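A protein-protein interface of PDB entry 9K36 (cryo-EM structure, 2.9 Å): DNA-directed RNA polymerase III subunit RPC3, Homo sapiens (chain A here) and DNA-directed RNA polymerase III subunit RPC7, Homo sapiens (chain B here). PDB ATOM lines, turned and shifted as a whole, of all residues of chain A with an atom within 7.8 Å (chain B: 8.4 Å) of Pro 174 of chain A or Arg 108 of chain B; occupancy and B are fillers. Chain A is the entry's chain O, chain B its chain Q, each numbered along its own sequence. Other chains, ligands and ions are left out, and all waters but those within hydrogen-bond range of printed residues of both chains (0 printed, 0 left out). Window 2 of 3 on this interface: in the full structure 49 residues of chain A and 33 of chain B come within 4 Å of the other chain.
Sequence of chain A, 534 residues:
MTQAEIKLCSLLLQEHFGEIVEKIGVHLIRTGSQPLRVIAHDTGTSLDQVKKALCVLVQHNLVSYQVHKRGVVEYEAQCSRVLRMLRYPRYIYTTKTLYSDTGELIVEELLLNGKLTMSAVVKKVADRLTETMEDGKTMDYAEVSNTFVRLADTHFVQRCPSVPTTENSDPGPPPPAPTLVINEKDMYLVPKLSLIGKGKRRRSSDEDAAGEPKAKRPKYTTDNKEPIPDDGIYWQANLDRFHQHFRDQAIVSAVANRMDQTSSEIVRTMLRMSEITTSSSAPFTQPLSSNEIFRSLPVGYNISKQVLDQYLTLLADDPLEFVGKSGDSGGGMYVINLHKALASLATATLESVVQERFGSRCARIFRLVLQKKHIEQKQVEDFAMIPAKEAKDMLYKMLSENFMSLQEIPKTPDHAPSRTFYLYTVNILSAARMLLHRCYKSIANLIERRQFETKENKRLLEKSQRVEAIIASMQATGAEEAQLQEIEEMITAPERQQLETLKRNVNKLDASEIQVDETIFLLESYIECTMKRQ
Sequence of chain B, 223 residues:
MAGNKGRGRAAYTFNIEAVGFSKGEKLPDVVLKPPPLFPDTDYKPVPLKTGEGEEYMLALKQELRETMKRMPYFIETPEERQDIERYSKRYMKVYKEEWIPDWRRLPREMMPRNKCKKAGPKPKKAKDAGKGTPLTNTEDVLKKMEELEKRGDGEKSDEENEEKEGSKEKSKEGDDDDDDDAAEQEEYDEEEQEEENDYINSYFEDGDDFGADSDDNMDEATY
Printed residues of chain B within 4 Å of Pro 174 of chain A: Arg 108.
Arg 108 of chain B touches just these residues of chain A: Pro 174 (2.7 Å), Pro 175 (3.3 Å) and Pro 176 (3.3 Å).
Pro 175 of chain A touches one residue of chain B.
Of the printed residues of chain A, Met 110 of chain B touches Leu 36, Lys 51 and Tyr 75.
Printed residues of chain B within 4 Å of Leu 36 of chain A: Glu 109 and Met 110.
Of the printed residues of chain B, Pro 178 of chain A touches Arg 104 and Arg 105.
Pro 171 of chain A touches none of the printed residues of chain B.
Pro 112 of chain B touches none of the printed residues of chain A.
The nearest printed residue of chain A that does not touch Met 111 of chain B is Leu 36 of chain A (7.5 Å).
O of Arg 108 of chain B is in hydrogen-bond range of NH1 of Arg 113 of chain B, 3.1 Å away.
The guanidinium group (NH1) of Arg 113 of chain B lies within hydrogen-bond range of the backbone carbonyl oxygen (O) of Met 111 of chain B (2.7 Å).
Of the 15 printed residues of chain A, 8 touch a printed residue of chain B.
Along chain A the printed residues that touch a printed residue of chain B span positions 36 to 178.
Among the printed residues, no Asp or Glu carboxylate lies within 4 Å of a Lys or Arg side-chain nitrogen of the other chain.
O of Pro 174 of chain A lies within hydrogen-bond range of NH2 of Arg 108 of chain B, 2.7 Å away.
O of Pro 176 of chain A lies within hydrogen-bond range of N of Arg 108 of chain B.
The backbone carbonyl oxygen (O) of Pro 175 of chain A lies within hydrogen-bond range of the guanidinium group (NH2) of Arg 108 of chain B, 3.3 Å away.
The side-chain amino group (NZ) of Lys 51 of chain A lies close to the guanidinium group (NH2) of Arg 113 of chain B (2.8 Å).
The side-chain hydroxyl of Tyr 75 of chain A sits at hydrogen-bond distance from the side-chain sulfur of Met 110 of chain B (2.8 Å).
Among the printed residues, merely in contact across the chains: Leu 36 of chain A with Glu 109 of chain B, Leu 36 of chain A with Met 110 of chain B, Lys 51 of chain A with Glu 109 of chain B, Lys 51 of chain A with Met 110 of chain B, Lys 51 of chain A with Met 111 of chain B, Val 73 of chain A with Glu 109 of chain B, Tyr 75 of chain A with Glu 109 of chain B, Pro 176 of chain A with Pro 107 of chain B, Pro 178 of chain A with Arg 104 of chain B and Pro 178 of chain A with Arg 105 of chain B.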
ATOM      1  N   LEU A  36      21.779   4.250  35.135  1.00  0.00           N
ATOM      2  CA  LEU A  36      20.892   3.230  34.582  1.00  0.00           C
ATOM      3  C   LEU A  36      21.140   1.865  35.214  1.00  0.00           C
ATOM      4  O   LEU A  36      20.194   1.114  35.481  1.00  0.00           O
ATOM      5  CB  LEU A  36      21.065   3.167  33.063  1.00  0.00           C
ATOM      6  CG  LEU A  36      20.007   2.451  32.217  1.00  0.00           C
ATOM      7  CD1 LEU A  36      19.985   3.041  30.818  1.00  0.00           C
ATOM      8  CD2 LEU A  36      20.265   0.954  32.141  1.00  0.00           C
ATOM      9  N   LYS A  51      15.591   0.132  29.682  1.00  0.00           N
ATOM     10  CA  LYS A  51      15.859   1.075  28.600  1.00  0.00           C
ATOM     11  C   LYS A  51      14.567   1.547  27.944  1.00  0.00           C
ATOM     12  O   LYS A  51      14.402   2.745  27.670  1.00  0.00           O
ATOM     13  CB  LYS A  51      16.783   0.433  27.566  1.00  0.00           C
ATOM     14  CG  LYS A  51      18.148   0.044  28.102  1.00  0.00           C
ATOM     15  CD  LYS A  51      18.951  -0.714  27.060  1.00  0.00           C
ATOM     16  CE  LYS A  51      20.286  -1.174  27.620  1.00  0.00           C
ATOM     17  NZ  LYS A  51      21.065  -1.963  26.626  1.00  0.00           N
ATOM     18  N   GLY A  71      31.816  10.942  32.971  1.00  0.00           N
ATOM     19  CA  GLY A  71      30.928  10.760  31.840  1.00  0.00           C
ATOM     20  C   GLY A  71      29.718   9.893  32.100  1.00  0.00           C
ATOM     21  O   GLY A  71      29.115   9.394  31.146  1.00  0.00           O
ATOM     22  N   VAL A  73      25.833   9.023  33.085  1.00  0.00           N
ATOM     23  CA  VAL A  73      24.538   9.653  32.857  1.00  0.00           C
ATOM     24  C   VAL A  73      23.600   9.258  33.989  1.00  0.00           C
ATOM     25  O   VAL A  73      23.500   8.076  34.343  1.00  0.00           O
ATOM     26  CB  VAL A  73      23.959   9.263  31.486  1.00  0.00           C
ATOM     27  CG1 VAL A  73      24.062   7.759  31.268  1.00  0.00           C
ATOM     28  CG2 VAL A  73      22.516   9.730  31.360  1.00  0.00           C
ATOM     29  N   TYR A  75      19.577   9.724  35.526  1.00  0.00           N
ATOM     30  CA  TYR A  75      18.202  10.025  35.155  1.00  0.00           C
ATOM     31  C   TYR A  75      17.428  10.469  36.389  1.00  0.00           C
ATOM     32  O   TYR A  75      17.417   9.764  37.404  1.00  0.00           O
ATOM     33  CB  TYR A  75      17.526   8.809  34.516  1.00  0.00           C
ATOM     34  CG  TYR A  75      18.280   8.238  33.339  1.00  0.00           C
ATOM     35  CD1 TYR A  75      18.081   8.733  32.056  1.00  0.00           C
ATOM     36  CD2 TYR A  75      19.189   7.203  33.506  1.00  0.00           C
ATOM     37  CE1 TYR A  75      18.768   8.212  30.976  1.00  0.00           C
ATOM     38  CE2 TYR A  75      19.879   6.676  32.432  1.00  0.00           C
ATOM     39  CZ  TYR A  75      19.665   7.185  31.169  1.00  0.00           C
ATOM     40  OH  TYR A  75      20.352   6.663  30.097  1.00  0.00           O
ATOM     41  N   THR A 166      26.915  18.756  16.457  1.00  0.00           N
ATOM     42  CA  THR A 166      28.053  17.941  16.864  1.00  0.00           C
ATOM     43  C   THR A 166      29.328  18.365  16.144  1.00  0.00           C
ATOM     44  O   THR A 166      30.423  18.284  16.711  1.00  0.00           O
ATOM     45  CB  THR A 166      27.760  16.462  16.608  1.00  0.00           C
ATOM     46  OG1 THR A 166      27.541  16.252  15.207  1.00  0.00           O
ATOM     47  CG2 THR A 166      26.525  16.024  17.381  1.00  0.00           C
ATOM     48  N   ASP A 170      32.767  20.643  19.697  1.00  0.00           N
ATOM     49  CA  ASP A 170      33.655  19.543  20.060  1.00  0.00           C
ATOM     50  C   ASP A 170      33.589  18.411  19.038  1.00  0.00           C
ATOM     51  O   ASP A 170      33.051  17.340  19.337  1.00  0.00           O
ATOM     52  CB  ASP A 170      33.309  19.018  21.456  1.00  0.00           C
ATOM     53  CG  ASP A 170      34.372  18.089  22.012  1.00  0.00           C
ATOM     54  OD1 ASP A 170      35.443  17.962  21.381  1.00  0.00           O
ATOM     55  OD2 ASP A 170      34.138  17.483  23.079  1.00  0.00           O
ATOM     56  N   PRO A 171      34.113  18.609  17.828  1.00  0.00           N
ATOM     57  CA  PRO A 171      34.118  17.518  16.845  1.00  0.00           C
ATOM     58  C   PRO A 171      35.126  16.444  17.236  1.00  0.00           C
ATOM     59  O   PRO A 171      36.300  16.734  17.479  1.00  0.00           O
ATOM     60  CB  PRO A 171      34.507  18.216  15.538  1.00  0.00           C
ATOM     61  CG  PRO A 171      35.313  19.393  15.979  1.00  0.00           C
ATOM     62  CD  PRO A 171      34.724  19.840  17.292  1.00  0.00           C
ATOM     63  N   GLY A 172      34.658  15.200  17.293  1.00  0.00           N
ATOM     64  CA  GLY A 172      35.505  14.089  17.657  1.00  0.00           C
ATOM     65  C   GLY A 172      34.736  12.962  18.314  1.00  0.00           C
ATOM     66  O   GLY A 172      33.729  12.474  17.789  1.00  0.00           O
ATOM     67  N   PRO A 173      35.205  12.515  19.476  1.00  0.00           N
ATOM     68  CA  PRO A 173      34.540  11.412  20.181  1.00  0.00           C
ATOM     69  C   PRO A 173      33.145  11.811  20.623  1.00  0.00           C
ATOM     70  O   PRO A 173      32.949  12.895  21.189  1.00  0.00           O
ATOM     71  CB  PRO A 173      35.457  11.157  21.389  1.00  0.00           C
ATOM     72  CG  PRO A 173      36.774  11.763  21.009  1.00  0.00           C
ATOM     73  CD  PRO A 173      36.434  12.947  20.163  1.00  0.00           C
ATOM     74  N   PRO A 174      32.151  10.960  20.390  1.00  0.00           N
ATOM     75  CA  PRO A 174      30.782  11.283  20.797  1.00  0.00           C
ATOM     76  C   PRO A 174      30.596  11.078  22.290  1.00  0.00           C
ATOM     77  O   PRO A 174      31.009  10.047  22.844  1.00  0.00           O
ATOM     78  CB  PRO A 174      29.932  10.297  19.987  1.00  0.00           C
ATOM     79  CG  PRO A 174      30.830   9.128  19.774  1.00  0.00           C
ATOM     80  CD  PRO A 174      32.226   9.687  19.648  1.00  0.00           C
ATOM     81  N   PRO A 175      29.987  12.039  22.979  1.00  0.00           N
ATOM     82  CA  PRO A 175      29.758  11.893  24.418  1.00  0.00           C
ATOM     83  C   PRO A 175      28.651  10.890  24.691  1.00  0.00           C
ATOM     84  O   PRO A 175      27.842  10.592  23.799  1.00  0.00           O
ATOM     85  CB  PRO A 175      29.350  13.306  24.854  1.00  0.00           C
ATOM     86  CG  PRO A 175      28.732  13.899  23.633  1.00  0.00           C
ATOM     87  CD  PRO A 175      29.498  13.331  22.468  1.00  0.00           C
ATOM     88  N   PRO A 176      28.591  10.335  25.906  1.00  0.00           N
ATOM     89  CA  PRO A 176      27.488   9.413  26.228  1.00  0.00           C
ATOM     90  C   PRO A 176      26.119  10.057  26.101  1.00  0.00           C
ATOM     91  O   PRO A 176      25.155   9.387  25.708  1.00  0.00           O
ATOM     92  CB  PRO A 176      27.793   8.998  27.674  1.00  0.00           C
ATOM     93  CG  PRO A 176      29.264   9.222  27.831  1.00  0.00           C
ATOM     94  CD  PRO A 176      29.574  10.427  26.999  1.00  0.00           C
ATOM     95  N   ALA A 177      26.006  11.343  26.424  1.00  0.00           N
ATOM     96  CA  ALA A 177      24.765  12.081  26.278  1.00  0.00           C
ATOM     97  C   ALA A 177      25.018  13.335  25.451  1.00  0.00           C
ATOM     98  O   ALA A 177      26.025  14.022  25.653  1.00  0.00           O
ATOM     99  CB  ALA A 177      24.181  12.465  27.645  1.00  0.00           C
ATOM    100  N   PRO A 178      24.120  13.657  24.512  1.00  0.00           N
ATOM    101  CA  PRO A 178      24.342  14.833  23.655  1.00  0.00           C
ATOM    102  C   PRO A 178      24.200  16.164  24.376  1.00  0.00           C
ATOM    103  O   PRO A 178      24.491  17.203  23.766  1.00  0.00           O
ATOM    104  CB  PRO A 178      23.278  14.675  22.563  1.00  0.00           C
ATOM    105  CG  PRO A 178      22.212  13.849  23.196  1.00  0.00           C
ATOM    106  CD  PRO A 178      22.903  12.916  24.144  1.00  0.00           C
ATOM    107  N   TRP B 103      17.215   8.491  18.482  1.00  0.00           N
ATOM    108  CA  TRP B 103      18.448   8.182  19.193  1.00  0.00           C
ATOM    109  C   TRP B 103      19.433   9.344  19.214  1.00  0.00           C
ATOM    110  O   TRP B 103      20.443   9.262  19.920  1.00  0.00           O
ATOM    111  CB  TRP B 103      19.111   6.952  18.572  1.00  0.00           C
ATOM    112  CG  TRP B 103      18.167   5.802  18.388  1.00  0.00           C
ATOM    113  CD1 TRP B 103      17.652   5.344  17.210  1.00  0.00           C
ATOM    114  CD2 TRP B 103      17.610   4.975  19.418  1.00  0.00           C
ATOM    115  NE1 TRP B 103      16.819   4.278  17.442  1.00  0.00           N
ATOM    116  CE2 TRP B 103      16.774   4.032  18.790  1.00  0.00           C
ATOM    117  CE3 TRP B 103      17.743   4.940  20.810  1.00  0.00           C
ATOM    118  CZ2 TRP B 103      16.072   3.063  19.503  1.00  0.00           C
ATOM    119  CZ3 TRP B 103      17.044   3.975  21.518  1.00  0.00           C
ATOM    120  CH2 TRP B 103      16.220   3.052  20.863  1.00  0.00           C
ATOM    121  N   ARG B 104      19.173  10.412  18.459  1.00  0.00           N
ATOM    122  CA  ARG B 104      20.054  11.576  18.498  1.00  0.00           C
ATOM    123  C   ARG B 104      19.948  12.296  19.837  1.00  0.00           C
ATOM    124  O   ARG B 104      20.965  12.682  20.426  1.00  0.00           O
ATOM    125  CB  ARG B 104      19.722  12.525  17.347  1.00  0.00           C
ATOM    126  CG  ARG B 104      19.883  11.907  15.968  1.00  0.00           C
ATOM    127  CD  ARG B 104      19.389  12.851  14.885  1.00  0.00           C
ATOM    128  NE  ARG B 104      17.972  13.163  15.044  1.00  0.00           N
ATOM    129  CZ  ARG B 104      17.291  13.970  14.237  1.00  0.00           C
ATOM    130  NH1 ARG B 104      17.896  14.551  13.210  1.00  0.00           N
ATOM    131  NH2 ARG B 104      16.002  14.196  14.458  1.00  0.00           N
ATOM    132  N   ARG B 105      18.724  12.483  20.335  1.00  0.00           N
ATOM    133  CA  ARG B 105      18.529  13.138  21.623  1.00  0.00           C
ATOM    134  C   ARG B 105      18.750  12.169  22.780  1.00  0.00           C
ATOM    135  O   ARG B 105      19.335  12.541  23.803  1.00  0.00           O
ATOM    136  CB  ARG B 105      17.126  13.739  21.695  1.00  0.00           C
ATOM    137  CG  ARG B 105      16.775  14.639  20.523  1.00  0.00           C
ATOM    138  CD  ARG B 105      15.292  14.968  20.503  1.00  0.00           C
ATOM    139  NE  ARG B 105      14.875  15.720  21.683  1.00  0.00           N
ATOM    140  CZ  ARG B 105      14.816  17.046  21.740  1.00  0.00           C
ATOM    141  NH1 ARG B 105      15.146  17.770  20.682  1.00  0.00           N
ATOM    142  NH2 ARG B 105      14.426  17.647  22.856  1.00  0.00           N
ATOM    143  N   LEU B 106      18.288  10.932  22.634  1.00  0.00           N
ATOM    144  CA  LEU B 106      18.441   9.947  23.692  1.00  0.00           C
ATOM    145  C   LEU B 106      19.889   9.467  23.759  1.00  0.00           C
ATOM    146  O   LEU B 106      20.519   9.246  22.719  1.00  0.00           O
ATOM    147  CB  LEU B 106      17.505   8.765  23.445  1.00  0.00           C
ATOM    148  CG  LEU B 106      17.322   7.715  24.541  1.00  0.00           C
ATOM    149  CD1 LEU B 106      16.673   8.325  25.773  1.00  0.00           C
ATOM    150  CD2 LEU B 106      16.486   6.559  24.017  1.00  0.00           C
ATOM    151  N   PRO B 107      20.449   9.310  24.958  1.00  0.00           N
ATOM    152  CA  PRO B 107      21.821   8.799  25.074  1.00  0.00           C
ATOM    153  C   PRO B 107      21.960   7.397  24.495  1.00  0.00           C
ATOM    154  O   PRO B 107      20.978   6.685  24.267  1.00  0.00           O
ATOM    155  CB  PRO B 107      22.079   8.808  26.585  1.00  0.00           C
ATOM    156  CG  PRO B 107      21.153   9.853  27.114  1.00  0.00           C
ATOM    157  CD  PRO B 107      19.924   9.778  26.254  1.00  0.00           C
ATOM    158  N   ARG B 108      23.215   7.004  24.265  1.00  0.00           N
ATOM    159  CA  ARG B 108      23.503   5.745  23.586  1.00  0.00           C
ATOM    160  C   ARG B 108      23.151   4.523  24.424  1.00  0.00           C
ATOM    161  O   ARG B 108      23.072   3.418  23.878  1.00  0.00           O
ATOM    162  CB  ARG B 108      24.981   5.681  23.199  1.00  0.00           C
ATOM    163  CG  ARG B 108      25.919   5.519  24.384  1.00  0.00           C
ATOM    164  CD  ARG B 108      27.302   5.069  23.940  1.00  0.00           C
ATOM    165  NE  ARG B 108      28.028   6.118  23.232  1.00  0.00           N
ATOM    166  CZ  ARG B 108      28.907   6.934  23.801  1.00  0.00           C
ATOM    167  NH1 ARG B 108      29.173   6.824  25.095  1.00  0.00           N
ATOM    168  NH2 ARG B 108      29.521   7.860  23.079  1.00  0.00           N
ATOM    169  N   GLU B 109      22.943   4.687  25.731  1.00  0.00           N
ATOM    170  CA  GLU B 109      22.774   3.537  26.611  1.00  0.00           C
ATOM    171  C   GLU B 109      21.423   2.851  26.463  1.00  0.00           C
ATOM    172  O   GLU B 109      21.244   1.765  27.025  1.00  0.00           O
ATOM    173  CB  GLU B 109      22.977   3.962  28.066  1.00  0.00           C
ATOM    174  CG  GLU B 109      24.376   4.473  28.374  1.00  0.00           C
ATOM    175  CD  GLU B 109      24.568   4.808  29.840  1.00  0.00           C
ATOM    176  OE1 GLU B 109      23.602   4.646  30.619  1.00  0.00           O
ATOM    177  OE2 GLU B 109      25.680   5.234  30.216  1.00  0.00           O
ATOM    178  N   MET B 110      20.474   3.440  25.737  1.00  0.00           N
ATOM    179  CA  MET B 110      19.135   2.873  25.617  1.00  0.00           C
ATOM    180  C   MET B 110      18.869   2.244  24.253  1.00  0.00           C
ATOM    181  O   MET B 110      17.719   1.897  23.959  1.00  0.00           O
ATOM    182  CB  MET B 110      18.077   3.936  25.915  1.00  0.00           C
ATOM    183  CG  MET B 110      17.826   4.171  27.395  1.00  0.00           C
ATOM    184  SD  MET B 110      19.268   4.821  28.256  1.00  0.00           S
ATOM    185  CE  MET B 110      19.526   6.349  27.364  1.00  0.00           C
ATOM    186  N   MET B 111      19.890   2.084  23.416  1.00  0.00           N
ATOM    187  CA  MET B 111      19.688   1.401  22.147  1.00  0.00           C
ATOM    188  C   MET B 111      19.549  -0.102  22.379  1.00  0.00           C
ATOM    189  O   MET B 111      20.247  -0.669  23.227  1.00  0.00           O
ATOM    190  CB  MET B 111      20.842   1.679  21.183  1.00  0.00           C
ATOM    191  CG  MET B 111      20.630   2.901  20.304  1.00  0.00           C
ATOM    192  SD  MET B 111      21.526   4.355  20.873  1.00  0.00           S
ATOM    193  CE  MET B 111      23.207   3.884  20.471  1.00  0.00           C
ATOM    194  N   PRO B 112      18.652  -0.774  21.652  1.00  0.00           N
ATOM    195  CA  PRO B 112      18.464  -2.215  21.878  1.00  0.00           C
ATOM    196  C   PRO B 112      19.650  -3.060  21.455  1.00  0.00           C
ATOM    197  O   PRO B 112      19.950  -4.061  22.119  1.00  0.00           O
ATOM    198  CB  PRO B 112      17.215  -2.541  21.041  1.00  0.00           C
ATOM    199  CG  PRO B 112      16.556  -1.216  20.781  1.00  0.00           C
ATOM    200  CD  PRO B 112      17.674  -0.230  20.699  1.00  0.00           C
ATOM    201  N   ARG B 113      20.334  -2.684  20.372  1.00  0.00           N
ATOM    202  CA  ARG B 113      21.421  -3.482  19.802  1.00  0.00           C
ATOM    203  C   ARG B 113      20.979  -4.918  19.533  1.00  0.00           C
ATOM    204  O   ARG B 113      21.456  -5.559  18.597  1.00  0.00           O
ATOM    205  CB  ARG B 113      22.651  -3.473  20.716  1.00  0.00           C
ATOM    206  CG  ARG B 113      23.485  -2.204  20.634  1.00  0.00           C
ATOM    207  CD  ARG B 113      23.059  -1.179  21.668  1.00  0.00           C
ATOM    208  NE  ARG B 113      23.383  -1.609  23.027  1.00  0.00           N
ATOM    209  CZ  ARG B 113      23.183  -0.870  24.111  1.00  0.00           C
ATOM    210  NH1 ARG B 113      22.657   0.343  24.003  1.00  0.00           N
ATOM    211  NH2 ARG B 113      23.505  -1.342  25.308  1.00  0.00           N
